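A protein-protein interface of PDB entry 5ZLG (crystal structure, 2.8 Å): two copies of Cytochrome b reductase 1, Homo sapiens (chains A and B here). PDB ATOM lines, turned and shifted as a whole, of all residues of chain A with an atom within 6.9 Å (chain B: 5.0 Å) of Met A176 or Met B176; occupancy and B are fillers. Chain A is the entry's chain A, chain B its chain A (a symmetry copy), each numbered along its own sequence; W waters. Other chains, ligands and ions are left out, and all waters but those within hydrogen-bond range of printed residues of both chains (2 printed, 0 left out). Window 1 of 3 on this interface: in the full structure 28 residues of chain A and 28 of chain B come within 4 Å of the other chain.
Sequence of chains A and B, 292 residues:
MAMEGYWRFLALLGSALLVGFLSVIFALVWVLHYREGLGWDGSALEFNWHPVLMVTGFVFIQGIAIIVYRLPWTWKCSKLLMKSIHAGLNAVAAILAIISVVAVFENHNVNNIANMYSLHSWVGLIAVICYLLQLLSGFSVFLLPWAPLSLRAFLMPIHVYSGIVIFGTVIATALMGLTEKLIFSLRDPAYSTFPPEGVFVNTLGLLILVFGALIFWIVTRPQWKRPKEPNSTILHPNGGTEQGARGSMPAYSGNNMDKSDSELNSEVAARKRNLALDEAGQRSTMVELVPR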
ATOM      1  N   SER A 118      33.131   8.157   1.074  1.00  0.00           N
ATOM      2  CA  SER A 118      32.005   8.253   0.168  1.00  0.00           C
ATOM      3  C   SER A 118      30.862   7.373   0.644  1.00  0.00           C
ATOM      4  O   SER A 118      31.042   6.442   1.427  1.00  0.00           O
ATOM      5  CB  SER A 118      32.425   7.850  -1.244  1.00  0.00           C
ATOM      6  OG  SER A 118      33.009   6.557  -1.229  1.00  0.00           O
ATOM      7  N   LEU A 119      29.667   7.691   0.160  1.00  0.00           N
ATOM      8  CA  LEU A 119      28.498   6.879   0.469  1.00  0.00           C
ATOM      9  C   LEU A 119      28.569   5.518  -0.212  1.00  0.00           C
ATOM     10  O   LEU A 119      28.088   4.515   0.337  1.00  0.00           O
ATOM     11  CB  LEU A 119      27.252   7.638   0.038  1.00  0.00           C
ATOM     12  CG  LEU A 119      25.864   7.054   0.214  1.00  0.00           C
ATOM     13  CD1 LEU A 119      25.570   6.842   1.689  1.00  0.00           C
ATOM     14  CD2 LEU A 119      24.865   8.008  -0.440  1.00  0.00           C
ATOM     15  N   HIS A 120      29.169   5.471  -1.403  1.00  0.00           N
ATOM     16  CA  HIS A 120      29.365   4.211  -2.108  1.00  0.00           C
ATOM     17  C   HIS A 120      30.234   3.255  -1.306  1.00  0.00           C
ATOM     18  O   HIS A 120      30.002   2.042  -1.318  1.00  0.00           O
ATOM     19  CB  HIS A 120      29.982   4.493  -3.475  1.00  0.00           C
ATOM     20  CG  HIS A 120      30.590   3.297  -4.141  1.00  0.00           C
ATOM     21  ND1 HIS A 120      29.911   2.536  -5.070  1.00  0.00           N
ATOM     22  CD2 HIS A 120      31.833   2.766  -4.056  1.00  0.00           C
ATOM     23  CE1 HIS A 120      30.704   1.576  -5.511  1.00  0.00           C
ATOM     24  NE2 HIS A 120      31.879   1.698  -4.921  1.00  0.00           N
ATOM     25  N   SER A 121      31.244   3.778  -0.606  1.00  0.00           N
ATOM     26  CA  SER A 121      32.089   2.914   0.208  1.00  0.00           C
ATOM     27  C   SER A 121      31.404   2.514   1.506  1.00  0.00           C
ATOM     28  O   SER A 121      31.604   1.396   1.991  1.00  0.00           O
ATOM     29  CB  SER A 121      33.417   3.596   0.505  1.00  0.00           C
ATOM     30  OG  SER A 121      33.221   4.957   0.815  1.00  0.00           O
ATOM     31  N   VAL A 123      27.968   2.151   2.104  1.00  0.00           N
ATOM     32  CA  VAL A 123      27.027   1.116   1.709  1.00  0.00           C
ATOM     33  C   VAL A 123      27.771  -0.132   1.243  1.00  0.00           C
ATOM     34  O   VAL A 123      27.532  -1.234   1.738  1.00  0.00           O
ATOM     35  CB  VAL A 123      26.082   1.667   0.634  1.00  0.00           C
ATOM     36  CG1 VAL A 123      25.130   0.584   0.158  1.00  0.00           C
ATOM     37  CG2 VAL A 123      25.347   2.911   1.191  1.00  0.00           C
ATOM     38  N   GLY A 124      28.712   0.031   0.313  1.00  0.00           N
ATOM     39  CA  GLY A 124      29.493  -1.108  -0.151  1.00  0.00           C
ATOM     40  C   GLY A 124      30.095  -1.943   0.967  1.00  0.00           C
ATOM     41  O   GLY A 124      30.002  -3.174   0.962  1.00  0.00           O
ATOM     42  N   VAL A 170      23.782  -4.391  -3.170  1.00  0.00           N
ATOM     43  CA  VAL A 170      24.975  -4.529  -3.997  1.00  0.00           C
ATOM     44  C   VAL A 170      24.730  -3.924  -5.369  1.00  0.00           C
ATOM     45  O   VAL A 170      25.617  -3.278  -5.941  1.00  0.00           O
ATOM     46  CB  VAL A 170      25.398  -6.009  -4.081  1.00  0.00           C
ATOM     47  CG1 VAL A 170      26.300  -6.246  -5.283  1.00  0.00           C
ATOM     48  CG2 VAL A 170      26.109  -6.411  -2.804  1.00  0.00           C
ATOM     49  N   ILE A 171      23.524  -4.111  -5.908  1.00  0.00           N
ATOM     50  CA  ILE A 171      23.171  -3.481  -7.179  1.00  0.00           C
ATOM     51  C   ILE A 171      23.220  -1.960  -7.048  1.00  0.00           C
ATOM     52  O   ILE A 171      23.770  -1.249  -7.902  1.00  0.00           O
ATOM     53  CB  ILE A 171      21.785  -3.964  -7.638  1.00  0.00           C
ATOM     54  CG1 ILE A 171      21.806  -5.477  -7.960  1.00  0.00           C
ATOM     55  CG2 ILE A 171      21.267  -3.100  -8.777  1.00  0.00           C
ATOM     56  CD1 ILE A 171      22.025  -5.847  -9.431  1.00  0.00           C
ATOM     57  N   ALA A 172      22.654  -1.444  -5.962  1.00  0.00           N
ATOM     58  CA  ALA A 172      22.653  -0.005  -5.741  1.00  0.00           C
ATOM     59  C   ALA A 172      24.065   0.531  -5.573  1.00  0.00           C
ATOM     60  O   ALA A 172      24.401   1.607  -6.093  1.00  0.00           O
ATOM     61  CB  ALA A 172      21.798   0.316  -4.521  1.00  0.00           C
ATOM     62  N   THR A 173      24.917  -0.212  -4.866  1.00  0.00           N
ATOM     63  CA  THR A 173      26.302   0.218  -4.714  1.00  0.00           C
ATOM     64  C   THR A 173      27.056   0.166  -6.034  1.00  0.00           C
ATOM     65  O   THR A 173      27.899   1.027  -6.287  1.00  0.00           O
ATOM     66  CB  THR A 173      27.015  -0.636  -3.681  1.00  0.00           C
ATOM     67  OG1 THR A 173      26.201  -0.732  -2.504  1.00  0.00           O
ATOM     68  CG2 THR A 173      28.356   0.006  -3.338  1.00  0.00           C
ATOM     69  N   ALA A 174      26.764  -0.822  -6.886  1.00  0.00           N
ATOM     70  CA  ALA A 174      27.360  -0.861  -8.221  1.00  0.00           C
ATOM     71  C   ALA A 174      27.016   0.390  -9.014  1.00  0.00           C
ATOM     72  O   ALA A 174      27.903   1.046  -9.580  1.00  0.00           O
ATOM     73  CB  ALA A 174      26.889  -2.098  -8.974  1.00  0.00           C
ATOM     74  N   LEU A 175      25.724   0.729  -9.073  1.00  0.00           N
ATOM     75  CA  LEU A 175      25.320   1.930  -9.801  1.00  0.00           C
ATOM     76  C   LEU A 175      25.966   3.184  -9.210  1.00  0.00           C
ATOM     77  O   LEU A 175      26.410   4.079  -9.948  1.00  0.00           O
ATOM     78  CB  LEU A 175      23.796   2.033  -9.810  1.00  0.00           C
ATOM     79  CG  LEU A 175      23.070   0.781 -10.308  1.00  0.00           C
ATOM     80  CD1 LEU A 175      21.589   1.039 -10.451  1.00  0.00           C
ATOM     81  CD2 LEU A 175      23.668   0.351 -11.621  1.00  0.00           C
ATOM     82  N   MET A 176      26.067   3.262  -7.885  1.00  0.00           N
ATOM     83  CA  MET A 176      26.819   4.376  -7.317  1.00  0.00           C
ATOM     84  C   MET A 176      28.275   4.347  -7.773  1.00  0.00           C
ATOM     85  O   MET A 176      28.858   5.395  -8.076  1.00  0.00           O
ATOM     86  CB  MET A 176      26.739   4.363  -5.794  1.00  0.00           C
ATOM     87  CG  MET A 176      25.445   4.904  -5.223  1.00  0.00           C
ATOM     88  SD  MET A 176      25.458   4.767  -3.411  1.00  0.00           S
ATOM     89  CE  MET A 176      26.559   6.060  -3.017  1.00  0.00           C
ATOM     90  N   GLY A 177      28.873   3.154  -7.845  1.00  0.00           N
ATOM     91  CA  GLY A 177      30.262   3.045  -8.276  1.00  0.00           C
ATOM     92  C   GLY A 177      30.476   3.548  -9.690  1.00  0.00           C
ATOM     93  O   GLY A 177      31.326   4.410  -9.938  1.00  0.00           O
ATOM     94  N   LEU A 178      29.684   3.030 -10.632  1.00  0.00           N
ATOM     95  CA  LEU A 178      29.690   3.546 -11.995  1.00  0.00           C
ATOM     96  C   LEU A 178      29.640   5.067 -12.004  1.00  0.00           C
ATOM     97  O   LEU A 178      30.521   5.716 -12.566  1.00  0.00           O
ATOM     98  CB  LEU A 178      28.517   2.958 -12.780  1.00  0.00           C
ATOM     99  CG  LEU A 178      28.595   1.459 -13.064  1.00  0.00           C
ATOM    100  CD1 LEU A 178      27.519   1.060 -14.048  1.00  0.00           C
ATOM    101  CD2 LEU A 178      29.970   1.070 -13.590  1.00  0.00           C
ATOM    102  N   THR A 179      28.629   5.653 -11.356  1.00  0.00           N
ATOM    103  CA  THR A 179      28.523   7.111 -11.300  1.00  0.00           C
ATOM    104  C   THR A 179      29.821   7.778 -10.845  1.00  0.00           C
ATOM    105  O   THR A 179      30.322   8.698 -11.509  1.00  0.00           O
ATOM    106  CB  THR A 179      27.380   7.501 -10.370  1.00  0.00           C
ATOM    107  OG1 THR A 179      26.153   7.387 -11.088  1.00  0.00           O
ATOM    108  CG2 THR A 179      27.545   8.935  -9.866  1.00  0.00           C
ATOM    109  N   GLU A 180      30.371   7.344  -9.701  1.00  0.00           N
ATOM    110  CA  GLU A 180      31.611   7.936  -9.200  1.00  0.00           C
ATOM    111  C   GLU A 180      32.705   7.887 -10.256  1.00  0.00           C
ATOM    112  O   GLU A 180      33.380   8.887 -10.524  1.00  0.00           O
ATOM    113  CB  GLU A 180      32.090   7.204  -7.946  1.00  0.00           C
ATOM    114  CG  GLU A 180      31.356   7.518  -6.659  1.00  0.00           C
ATOM    115  CD  GLU A 180      32.129   7.027  -5.436  1.00  0.00           C
ATOM    116  OE1 GLU A 180      33.094   6.238  -5.608  1.00  0.00           O
ATOM    117  OE2 GLU A 180      31.779   7.443  -4.309  1.00  0.00           O
ATOM    118  N   LYS A 181      32.884   6.713 -10.866  1.00  0.00           N
ATOM    119  CA  LYS A 181      33.964   6.517 -11.828  1.00  0.00           C
ATOM    120  C   LYS A 181      33.791   7.400 -13.058  1.00  0.00           C
ATOM    121  O   LYS A 181      34.752   8.030 -13.514  1.00  0.00           O
ATOM    122  CB  LYS A 181      34.029   5.051 -12.237  1.00  0.00           C
ATOM    123  CG  LYS A 181      35.228   4.719 -13.080  1.00  0.00           C
ATOM    124  CD  LYS A 181      36.512   5.192 -12.421  1.00  0.00           C
ATOM    125  CE  LYS A 181      37.704   4.871 -13.292  1.00  0.00           C
ATOM    126  NZ  LYS A 181      38.958   5.066 -12.533  1.00  0.00           N
ATOM    127  N   ILE A 183      32.057  10.221 -13.301  1.00  0.00           N
ATOM    128  CA  ILE A 183      32.194  11.636 -12.968  1.00  0.00           C
ATOM    129  C   ILE A 183      33.657  11.996 -12.739  1.00  0.00           C
ATOM    130  O   ILE A 183      34.146  13.017 -13.237  1.00  0.00           O
ATOM    131  CB  ILE A 183      31.334  11.986 -11.745  1.00  0.00           C
ATOM    132  CG1 ILE A 183      29.851  11.884 -12.091  1.00  0.00           C
ATOM    133  CG2 ILE A 183      31.657  13.390 -11.248  1.00  0.00           C
ATOM    134  CD1 ILE A 183      28.970  12.298 -10.965  1.00  0.00           C
ATOM    135  N   TYR A 191      31.671  13.969 -19.114  1.00  0.00           N
ATOM    136  CA  TYR A 191      30.468  13.143 -19.010  1.00  0.00           C
ATOM    137  C   TYR A 191      29.250  13.846 -19.605  1.00  0.00           C
ATOM    138  O   TYR A 191      28.472  13.243 -20.351  1.00  0.00           O
ATOM    139  CB  TYR A 191      30.226  12.817 -17.534  1.00  0.00           C
ATOM    140  CG  TYR A 191      29.316  11.654 -17.195  1.00  0.00           C
ATOM    141  CD1 TYR A 191      28.966  10.686 -18.134  1.00  0.00           C
ATOM    142  CD2 TYR A 191      28.820  11.520 -15.908  1.00  0.00           C
ATOM    143  CE1 TYR A 191      28.134   9.618 -17.783  1.00  0.00           C
ATOM    144  CE2 TYR A 191      28.000  10.469 -15.556  1.00  0.00           C
ATOM    145  CZ  TYR A 191      27.655   9.522 -16.484  1.00  0.00           C
ATOM    146  OH  TYR A 191      26.819   8.491 -16.086  1.00  0.00           O
ATOM    147  N   LEU B 119      23.779   8.199 -15.651  1.00  0.00           N
ATOM    148  CA  LEU B 119      23.080   6.962 -15.330  1.00  0.00           C
ATOM    149  C   LEU B 119      21.980   7.194 -14.301  1.00  0.00           C
ATOM    150  O   LEU B 119      20.937   6.525 -14.337  1.00  0.00           O
ATOM    151  CB  LEU B 119      24.095   5.949 -14.821  1.00  0.00           C
ATOM    152  CG  LEU B 119      23.680   4.556 -14.389  1.00  0.00           C
ATOM    153  CD1 LEU B 119      23.091   3.799 -15.566  1.00  0.00           C
ATOM    154  CD2 LEU B 119      24.910   3.855 -13.813  1.00  0.00           C
ATOM    155  N   HIS B 120      22.200   8.140 -13.387  1.00  0.00           N
ATOM    156  CA  HIS B 120      21.185   8.503 -12.407  1.00  0.00           C
ATOM    157  C   HIS B 120      19.928   9.032 -13.077  1.00  0.00           C
ATOM    158  O   HIS B 120      18.815   8.770 -12.611  1.00  0.00           O
ATOM    159  CB  HIS B 120      21.766   9.534 -11.443  1.00  0.00           C
ATOM    160  CG  HIS B 120      20.745  10.276 -10.637  1.00  0.00           C
ATOM    161  ND1 HIS B 120      20.388   9.900  -9.359  1.00  0.00           N
ATOM    162  CD2 HIS B 120      20.047  11.406 -10.906  1.00  0.00           C
ATOM    163  CE1 HIS B 120      19.498  10.756  -8.885  1.00  0.00           C
ATOM    164  NE2 HIS B 120      19.281  11.684  -9.799  1.00  0.00           N
ATOM    165  N   VAL B 123      18.200   5.756 -15.140  1.00  0.00           N
ATOM    166  CA  VAL B 123      17.464   4.950 -14.180  1.00  0.00           C
ATOM    167  C   VAL B 123      16.316   5.755 -13.578  1.00  0.00           C
ATOM    168  O   VAL B 123      15.161   5.329 -13.603  1.00  0.00           O
ATOM    169  CB  VAL B 123      18.428   4.421 -13.111  1.00  0.00           C
ATOM    170  CG1 VAL B 123      17.670   3.629 -12.060  1.00  0.00           C
ATOM    171  CG2 VAL B 123      19.544   3.595 -13.797  1.00  0.00           C
ATOM    172  N   ALA B 172      17.870   3.161  -5.172  1.00  0.00           N
ATOM    173  CA  ALA B 172      19.169   3.144  -5.830  1.00  0.00           C
ATOM    174  C   ALA B 172      19.434   4.448  -6.564  1.00  0.00           C
ATOM    175  O   ALA B 172      20.559   4.974  -6.537  1.00  0.00           O
ATOM    176  CB  ALA B 172      19.234   1.958  -6.784  1.00  0.00           C
ATOM    177  N   THR B 173      18.408   5.000  -7.213  1.00  0.00           N
ATOM    178  CA  THR B 173      18.582   6.280  -7.890  1.00  0.00           C
ATOM    179  C   THR B 173      18.814   7.413  -6.902  1.00  0.00           C
ATOM    180  O   THR B 173      19.587   8.326  -7.194  1.00  0.00           O
ATOM    181  CB  THR B 173      17.376   6.593  -8.756  1.00  0.00           C
ATOM    182  OG1 THR B 173      17.053   5.442  -9.550  1.00  0.00           O
ATOM    183  CG2 THR B 173      17.700   7.777  -9.661  1.00  0.00           C
ATOM    184  N   ALA B 174      18.166   7.371  -5.734  1.00  0.00           N
ATOM    185  CA  ALA B 174      18.437   8.360  -4.691  1.00  0.00           C
ATOM    186  C   ALA B 174      19.898   8.336  -4.274  1.00  0.00           C
ATOM    187  O   ALA B 174      20.564   9.381  -4.231  1.00  0.00           O
ATOM    188  CB  ALA B 174      17.549   8.107  -3.479  1.00  0.00           C
ATOM    189  N   LEU B 175      20.414   7.144  -3.954  1.00  0.00           N
ATOM    190  CA  LEU B 175      21.818   7.041  -3.563  1.00  0.00           C
ATOM    191  C   LEU B 175      22.745   7.512  -4.684  1.00  0.00           C
ATOM    192  O   LEU B 175      23.747   8.202  -4.433  1.00  0.00           O
ATOM    193  CB  LEU B 175      22.127   5.604  -3.144  1.00  0.00           C
ATOM    194  CG  LEU B 175      21.185   5.028  -2.084  1.00  0.00           C
ATOM    195  CD1 LEU B 175      21.674   3.681  -1.606  1.00  0.00           C
ATOM    196  CD2 LEU B 175      21.079   5.996  -0.936  1.00  0.00           C
ATOM    197  N   MET B 176      22.419   7.187  -5.934  1.00  0.00           N
ATOM    198  CA  MET B 176      23.206   7.761  -7.020  1.00  0.00           C
ATOM    199  C   MET B 176      23.113   9.284  -7.023  1.00  0.00           C
ATOM    200  O   MET B 176      24.113   9.973  -7.255  1.00  0.00           O
ATOM    201  CB  MET B 176      22.761   7.199  -8.366  1.00  0.00           C
ATOM    202  CG  MET B 176      23.284   5.812  -8.677  1.00  0.00           C
ATOM    203  SD  MET B 176      22.625   5.240 -10.272  1.00  0.00           S
ATOM    204  CE  MET B 176      23.585   6.207 -11.360  1.00  0.00           C
ATOM    205  N   GLY B 177      21.922   9.828  -6.752  1.00  0.00           N
ATOM    206  CA  GLY B 177      21.754  11.276  -6.732  1.00  0.00           C
ATOM    207  C   GLY B 177      22.613  11.950  -5.680  1.00  0.00           C
ATOM    208  O   GLY B 177      23.385  12.867  -5.979  1.00  0.00           O
ATOM    209  N   LEU B 178      22.505  11.480  -4.435  1.00  0.00           N
ATOM    210  CA  LEU B 178      23.390  11.941  -3.372  1.00  0.00           C
ATOM    211  C   LEU B 178      24.839  11.955  -3.835  1.00  0.00           C
ATOM    212  O   LEU B 178      25.497  12.994  -3.791  1.00  0.00           O
ATOM    213  CB  LEU B 178      23.221  11.058  -2.134  1.00  0.00           C
ATOM    214  CG  LEU B 178      21.874  11.165  -1.423  1.00  0.00           C
ATOM    215  CD1 LEU B 178      21.929  10.445  -0.095  1.00  0.00           C
ATOM    216  CD2 LEU B 178      21.471  12.620  -1.224  1.00  0.00           C
ATOM    217  N   THR B 179      25.343  10.814  -4.312  1.00  0.00           N
ATOM    218  CA  THR B 179      26.722  10.752  -4.797  1.00  0.00           C
ATOM    219  C   THR B 179      27.044  11.862  -5.798  1.00  0.00           C
ATOM    220  O   THR B 179      28.040  12.583  -5.639  1.00  0.00           O
ATOM    221  CB  THR B 179      26.977   9.388  -5.428  1.00  0.00           C
ATOM    222  OG1 THR B 179      27.246   8.451  -4.387  1.00  0.00           O
ATOM    223  CG2 THR B 179      28.165   9.439  -6.388  1.00  0.00           C
ATOM    224  N   GLU B 180      26.225  12.000  -6.851  1.00  0.00           N
ATOM    225  CA  GLU B 180      26.470  13.037  -7.854  1.00  0.00           C
ATOM    226  C   GLU B 180      26.581  14.408  -7.204  1.00  0.00           C
ATOM    227  O   GLU B 180      27.514  15.172  -7.478  1.00  0.00           O
ATOM    228  CB  GLU B 180      25.347  13.063  -8.890  1.00  0.00           C
ATOM    229  CG  GLU B 180      25.369  11.968  -9.937  1.00  0.00           C
ATOM    230  CD  GLU B 180      24.443  12.290 -11.109  1.00  0.00           C
ATOM    231  OE1 GLU B 180      23.614  13.229 -10.982  1.00  0.00           O
ATOM    232  OE2 GLU B 180      24.557  11.616 -12.156  1.00  0.00           O
HETATM  233  O   HOH W   1      24.901   8.809 -12.623  1.00  0.00           O
HETATM  234  O   HOH W   2      29.211   7.810  -3.092  1.00  0.00           O
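OH of Tyr A191 lies within hydrogen-bond range of N of Leu B119 (3.1 Å).
The side-chain hydroxyl (OG) of Ser A118 sits close to the side-chain carboxylate (OE2) of Glu A180 (3.4 Å).
Among the printed residues, pairs that only touch across the chains: Thr A179 with Met B176 (2.8 Å), Met A176 with Thr B179 (2.8 Å), Met A176 with Leu B175 (3.4 Å), Leu A175 with Met B176 (3.4 Å), Thr A179 with Thr B179 (3.6 Å), Thr A179 with Glu B180 (3.7 Å), Glu A180 with Thr B179 (3.7 Å), Ile A183 with Glu B180 (3.8 Å), Ala A172 with Ala B172 (3.8 Å), Leu A178 with Leu B119 (3.8 Å), Leu A119 with Leu B178 (3.8 Å) and Met A176 with Met B176 (3.9 Å).
Of chain B, only Leu B175, Met B176 and Thr B179 come within 4 Å of Met A176. Printed residues of chain A within 4 Å of Ala B172: Ala A172 (3.8 Å). Printed residues of chain A within 4 Å of Leu B119: Leu A178 (3.8 Å) and Tyr A191 (3.1 Å). Of the printed residues of chain A, Glu B180 touches Thr A179 (3.7 Å) and Ile A183 (3.8 Å). The nearest printed residue of chain B that does not touch Met A176 is Ala B172 (5.1 Å). The nearest residue of chain A that does not touch Met B176 is Ala A172 (5.1 Å).
Of the 12 printed residues of chain B, 7 touch a printed residue of chain A. Hydrophobic or aromatic side chains of chain B within 4 Å of the printed part of chain A: Leu B119, Ala B172, Leu B175, Met B176 and Leu B178. Along chain B the printed residues that touch a printed residue of chain A span positions 119 to 180. Of the 20 printed residues of chain A, 9 touch a printed residue of chain B. Printed residues of chain A that touch a printed residue of chain B: Leu A119, Ala A172, Leu A175, Met A176, Leu A178, Thr A179, Glu A180, Ile A183 and Tyr A191. Hydrophobic or aromatic side chains of chain A within 4 Å of the printed part of chain B: Leu A119, Ala A172, Leu A175, Met A176, Leu A178, Ile A183 and Tyr A191. Among the printed residues, 13 pairs touch across the chains. Among the printed residues, no Asp or Glu carboxylate lies within 4 Å of a Lys or Arg side-chain nitrogen of the other chain.
Leu A119 touches Leu B178, and with the chains exchanged Leu A178 touches Leu B119. Met A176 touches its own counterpart, Met B176. Thr A179 touches its own counterpart, Thr B179. Thr A179 touches Glu B180, and with the chains exchanged Glu A180 touches Thr B179.
Water W1 lies within hydrogen-bond range of OG1 of Thr A179, OE2 of Glu B180, N of His B120 and N of Leu B119. Water W2 lies within hydrogen-bond range of the side-chain hydroxyl (OG1) of Thr B179 (2.4 Å), the side-chain carboxylate (OE2) of Glu A180 (2.9 Å), the backbone NH (N) of His A120 (2.9 Å) and the backbone NH (N) of Leu A119 (3.3 Å).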
